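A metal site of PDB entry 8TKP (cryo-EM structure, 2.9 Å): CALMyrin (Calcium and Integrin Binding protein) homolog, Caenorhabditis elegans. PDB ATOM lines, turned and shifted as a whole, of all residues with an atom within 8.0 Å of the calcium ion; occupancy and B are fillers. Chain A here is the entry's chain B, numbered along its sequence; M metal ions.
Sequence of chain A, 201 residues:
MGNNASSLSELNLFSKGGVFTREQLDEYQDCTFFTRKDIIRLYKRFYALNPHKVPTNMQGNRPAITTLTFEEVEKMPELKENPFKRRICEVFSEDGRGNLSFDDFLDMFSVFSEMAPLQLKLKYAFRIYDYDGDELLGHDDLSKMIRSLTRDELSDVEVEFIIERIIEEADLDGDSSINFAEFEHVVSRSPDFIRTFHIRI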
ATOM      1  N   PHE A 126      13.109  34.726  32.523  1.00  0.00           N
ATOM      2  CA  PHE A 126      12.706  34.084  31.271  1.00  0.00           C
ATOM      3  C   PHE A 126      13.474  32.793  31.055  1.00  0.00           C
ATOM      4  O   PHE A 126      12.908  31.785  30.615  1.00  0.00           O
ATOM      5  CB  PHE A 126      12.906  35.040  30.105  1.00  0.00           C
ATOM      6  CG  PHE A 126      12.424  34.501  28.789  1.00  0.00           C
ATOM      7  CD1 PHE A 126      11.120  34.688  28.390  1.00  0.00           C
ATOM      8  CD2 PHE A 126      13.288  33.810  27.942  1.00  0.00           C
ATOM      9  CE1 PHE A 126      10.673  34.191  27.181  1.00  0.00           C
ATOM     10  CE2 PHE A 126      12.842  33.307  26.741  1.00  0.00           C
ATOM     11  CZ  PHE A 126      11.527  33.507  26.357  1.00  0.00           C
ATOM     12  N   TYR A 129      12.001  30.118  33.520  1.00  0.00           N
ATOM     13  CA  TYR A 129      10.699  29.590  33.139  1.00  0.00           C
ATOM     14  C   TYR A 129      10.726  28.860  31.808  1.00  0.00           C
ATOM     15  O   TYR A 129       9.742  28.197  31.462  1.00  0.00           O
ATOM     16  CB  TYR A 129       9.673  30.735  33.084  1.00  0.00           C
ATOM     17  CG  TYR A 129       9.497  31.442  34.410  1.00  0.00           C
ATOM     18  CD1 TYR A 129       9.665  30.766  35.604  1.00  0.00           C
ATOM     19  CD2 TYR A 129       9.181  32.789  34.463  1.00  0.00           C
ATOM     20  CE1 TYR A 129       9.519  31.408  36.811  1.00  0.00           C
ATOM     21  CE2 TYR A 129       9.033  33.444  35.669  1.00  0.00           C
ATOM     22  CZ  TYR A 129       9.203  32.747  36.843  1.00  0.00           C
ATOM     23  OH  TYR A 129       9.057  33.388  38.050  1.00  0.00           O
ATOM     24  N   ASP A 130      11.826  28.939  31.059  1.00  0.00           N
ATOM     25  CA  ASP A 130      11.971  28.222  29.801  1.00  0.00           C
ATOM     26  C   ASP A 130      12.556  26.839  30.074  1.00  0.00           C
ATOM     27  O   ASP A 130      13.762  26.598  29.966  1.00  0.00           O
ATOM     28  CB  ASP A 130      12.838  29.029  28.830  1.00  0.00           C
ATOM     29  CG  ASP A 130      12.813  28.465  27.428  1.00  0.00           C
ATOM     30  OD1 ASP A 130      11.715  28.097  26.950  1.00  0.00           O
ATOM     31  OD2 ASP A 130      13.881  28.413  26.792  1.00  0.00           O
ATOM     32  N   TYR A 131      11.666  25.924  30.471  1.00  0.00           N
ATOM     33  CA  TYR A 131      12.081  24.585  30.856  1.00  0.00           C
ATOM     34  C   TYR A 131      12.785  23.859  29.715  1.00  0.00           C
ATOM     35  O   TYR A 131      13.877  23.313  29.876  1.00  0.00           O
ATOM     36  CB  TYR A 131      10.870  23.774  31.327  1.00  0.00           C
ATOM     37  CG  TYR A 131      10.335  24.184  32.675  1.00  0.00           C
ATOM     38  CD1 TYR A 131       9.521  25.302  32.808  1.00  0.00           C
ATOM     39  CD2 TYR A 131      10.622  23.443  33.805  1.00  0.00           C
ATOM     40  CE1 TYR A 131       9.021  25.677  34.048  1.00  0.00           C
ATOM     41  CE2 TYR A 131      10.124  23.810  35.038  1.00  0.00           C
ATOM     42  CZ  TYR A 131       9.328  24.924  35.149  1.00  0.00           C
ATOM     43  OH  TYR A 131       8.841  25.288  36.388  1.00  0.00           O
ATOM     44  N   ASP A 132      12.161  23.848  28.530  1.00  0.00           N
ATOM     45  CA  ASP A 132      12.715  23.107  27.405  1.00  0.00           C
ATOM     46  C   ASP A 132      13.979  23.758  26.848  1.00  0.00           C
ATOM     47  O   ASP A 132      14.709  23.116  26.082  1.00  0.00           O
ATOM     48  CB  ASP A 132      11.666  22.962  26.307  1.00  0.00           C
ATOM     49  CG  ASP A 132      10.933  24.257  26.028  1.00  0.00           C
ATOM     50  OD1 ASP A 132      11.306  25.290  26.613  1.00  0.00           O
ATOM     51  OD2 ASP A 132       9.966  24.231  25.227  1.00  0.00           O
ATOM     52  N   GLY A 133      14.241  25.010  27.207  1.00  0.00           N
ATOM     53  CA  GLY A 133      15.433  25.692  26.712  1.00  0.00           C
ATOM     54  C   GLY A 133      15.427  25.959  25.225  1.00  0.00           C
ATOM     55  O   GLY A 133      16.470  25.807  24.564  1.00  0.00           O
ATOM     56  N   ASP A 134      14.287  26.367  24.673  1.00  0.00           N
ATOM     57  CA  ASP A 134      14.177  26.680  23.258  1.00  0.00           C
ATOM     58  C   ASP A 134      13.941  28.164  22.986  1.00  0.00           C
ATOM     59  O   ASP A 134      13.452  28.520  21.918  1.00  0.00           O
ATOM     60  CB  ASP A 134      13.060  25.852  22.616  1.00  0.00           C
ATOM     61  CG  ASP A 134      11.714  26.079  23.280  1.00  0.00           C
ATOM     62  OD1 ASP A 134      11.662  26.809  24.293  1.00  0.00           O
ATOM     63  OD2 ASP A 134      10.713  25.521  22.786  1.00  0.00           O
ATOM     64  N   GLU A 135      14.260  29.020  23.961  1.00  0.00           N
ATOM     65  CA  GLU A 135      14.263  30.491  23.880  1.00  0.00           C
ATOM     66  C   GLU A 135      12.848  31.087  23.855  1.00  0.00           C
ATOM     67  O   GLU A 135      12.734  32.308  23.740  1.00  0.00           O
ATOM     68  CB  GLU A 135      15.049  31.001  22.661  1.00  0.00           C
ATOM     69  CG  GLU A 135      15.650  32.399  22.834  1.00  0.00           C
ATOM     70  CD  GLU A 135      14.878  33.472  22.076  1.00  0.00           C
ATOM     71  OE1 GLU A 135      14.253  33.136  21.044  1.00  0.00           O
ATOM     72  OE2 GLU A 135      14.880  34.631  22.525  1.00  0.00           O
ATOM     73  N   LEU A 136      11.788  30.287  23.954  1.00  0.00           N
ATOM     74  CA  LEU A 136      10.445  30.822  24.004  1.00  0.00           C
ATOM     75  C   LEU A 136       9.598  30.012  24.966  1.00  0.00           C
ATOM     76  O   LEU A 136       9.695  28.784  25.011  1.00  0.00           O
ATOM     77  CB  LEU A 136       9.798  30.853  22.605  1.00  0.00           C
ATOM     78  CG  LEU A 136      10.092  29.739  21.596  1.00  0.00           C
ATOM     79  CD1 LEU A 136       9.327  28.463  21.915  1.00  0.00           C
ATOM     80  CD2 LEU A 136       9.764  30.225  20.189  1.00  0.00           C
ATOM     81  N   LEU A 137       8.767  30.706  25.752  1.00  0.00           N
ATOM     82  CA  LEU A 137       7.890  30.049  26.720  1.00  0.00           C
ATOM     83  C   LEU A 137       6.717  29.442  25.975  1.00  0.00           C
ATOM     84  O   LEU A 137       5.772  30.144  25.582  1.00  0.00           O
ATOM     85  CB  LEU A 137       7.422  31.035  27.776  1.00  0.00           C
ATOM     86  CG  LEU A 137       8.498  31.791  28.555  1.00  0.00           C
ATOM     87  CD1 LEU A 137       7.869  32.665  29.628  1.00  0.00           C
ATOM     88  CD2 LEU A 137       9.497  30.836  29.161  1.00  0.00           C
ATOM     89  N   GLY A 138       6.761  28.131  25.761  1.00  0.00           N
ATOM     90  CA  GLY A 138       5.720  27.436  25.038  1.00  0.00           C
ATOM     91  C   GLY A 138       4.517  27.118  25.907  1.00  0.00           C
ATOM     92  O   GLY A 138       4.364  27.595  27.027  1.00  0.00           O
ATOM     93  N   HIS A 139       3.650  26.273  25.356  1.00  0.00           N
ATOM     94  CA  HIS A 139       2.436  25.873  26.075  1.00  0.00           C
ATOM     95  C   HIS A 139       2.779  24.996  27.274  1.00  0.00           C
ATOM     96  O   HIS A 139       2.282  25.226  28.375  1.00  0.00           O
ATOM     97  CB  HIS A 139       1.489  25.142  25.118  1.00  0.00           C
ATOM     98  CG  HIS A 139       0.303  24.528  25.792  1.00  0.00           C
ATOM     99  ND1 HIS A 139       0.341  23.271  26.344  1.00  0.00           N
ATOM    100  CD2 HIS A 139      -0.946  24.989  25.995  1.00  0.00           C
ATOM    101  CE1 HIS A 139      -0.835  22.984  26.866  1.00  0.00           C
ATOM    102  NE2 HIS A 139      -1.640  24.014  26.663  1.00  0.00           N
ATOM    103  N   ASP A 140       3.624  23.988  27.066  1.00  0.00           N
ATOM    104  CA  ASP A 140       3.924  23.052  28.145  1.00  0.00           C
ATOM    105  C   ASP A 140       4.728  23.711  29.257  1.00  0.00           C
ATOM    106  O   ASP A 140       4.566  23.342  30.433  1.00  0.00           O
ATOM    107  CB  ASP A 140       4.679  21.841  27.597  1.00  0.00           C
ATOM    108  CG  ASP A 140       5.995  22.230  26.948  1.00  0.00           C
ATOM    109  OD1 ASP A 140       6.100  23.359  26.434  1.00  0.00           O
ATOM    110  OD2 ASP A 140       6.934  21.390  26.953  1.00  0.00           O
ATOM    111  N   ASP A 141       5.597  24.668  28.930  1.00  0.00           N
ATOM    112  CA  ASP A 141       6.327  25.394  29.959  1.00  0.00           C
ATOM    113  C   ASP A 141       5.378  26.144  30.881  1.00  0.00           C
ATOM    114  O   ASP A 141       5.489  26.080  32.107  1.00  0.00           O
ATOM    115  CB  ASP A 141       7.325  26.355  29.327  1.00  0.00           C
ATOM    116  CG  ASP A 141       8.369  25.644  28.493  1.00  0.00           C
ATOM    117  OD1 ASP A 141       8.740  24.503  28.847  1.00  0.00           O
ATOM    118  OD2 ASP A 141       8.817  26.218  27.481  1.00  0.00           O
ATOM    119  N   LEU A 142       4.410  26.853  30.297  1.00  0.00           N
ATOM    120  CA  LEU A 142       3.419  27.544  31.099  1.00  0.00           C
ATOM    121  C   LEU A 142       2.577  26.560  31.895  1.00  0.00           C
ATOM    122  O   LEU A 142       2.226  26.817  33.058  1.00  0.00           O
ATOM    123  CB  LEU A 142       2.519  28.402  30.205  1.00  0.00           C
ATOM    124  CG  LEU A 142       3.212  29.507  29.393  1.00  0.00           C
ATOM    125  CD1 LEU A 142       2.218  30.215  28.491  1.00  0.00           C
ATOM    126  CD2 LEU A 142       3.907  30.495  30.306  1.00  0.00           C
ATOM    127  N   SER A 177       3.485  31.303  21.205  1.00  0.00           N
ATOM    128  CA  SER A 177       4.544  31.243  22.202  1.00  0.00           C
ATOM    129  C   SER A 177       5.013  32.657  22.508  1.00  0.00           C
ATOM    130  O   SER A 177       4.810  33.578  21.712  1.00  0.00           O
ATOM    131  CB  SER A 177       5.712  30.375  21.738  1.00  0.00           C
ATOM    132  OG  SER A 177       6.237  30.852  20.511  1.00  0.00           O
ATOM    133  N   ILE A 178       5.634  32.818  23.660  1.00  0.00           N
ATOM    134  CA  ILE A 178       6.067  34.113  24.156  1.00  0.00           C
ATOM    135  C   ILE A 178       7.577  34.204  23.966  1.00  0.00           C
ATOM    136  O   ILE A 178       8.342  33.563  24.693  1.00  0.00           O
ATOM    137  CB  ILE A 178       5.676  34.334  25.625  1.00  0.00           C
ATOM    138  CG1 ILE A 178       4.170  34.163  25.800  1.00  0.00           C
ATOM    139  CG2 ILE A 178       6.108  35.713  26.086  1.00  0.00           C
ATOM    140  CD1 ILE A 178       3.706  34.316  27.231  1.00  0.00           C
HETATM  141 CA    CA M   1       9.695  26.506  25.421  1.00  0.00          CA
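The side-chain carboxylate (OD2) of Asp 130 lies within hydrogen-bond range of the backbone NH (N) of Asp 134, 3.0 Å away. OD2 of Asp 141 sits close to N of Gly 138 (3.3 Å). The side-chain carboxylate (OD2) of Asp 130 lies close to the backbone NH (N) of Gly 133 (3.4 Å). The side-chain carboxylate (OD2) of Asp 130 lies within hydrogen-bond range of the backbone NH (N) of Glu 135, 2.9 Å away.
Merely in contact with the calcium ion: Gly 138. The nearest printed residue that does not touch the calcium ion is Leu 137 (4.2 Å).
The calcium ion is bound by OD2 of Asp 141 (2.3 Å), OD1 of Asp 134 (2.3 Å), OD2 of Asp 132 (2.3 Å), O of Leu 136 (2.3 Å) and OD1 of Asp 132 (2.3 Å). The calcium ion has five donor atoms within binding distance. Slightly farther from the calcium ion lies OD1 of Asp 130 (3.0 Å). Slightly farther from the calcium ion lies the side-chain carboxylate (OD2) of Asp 134 (3.0 Å).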
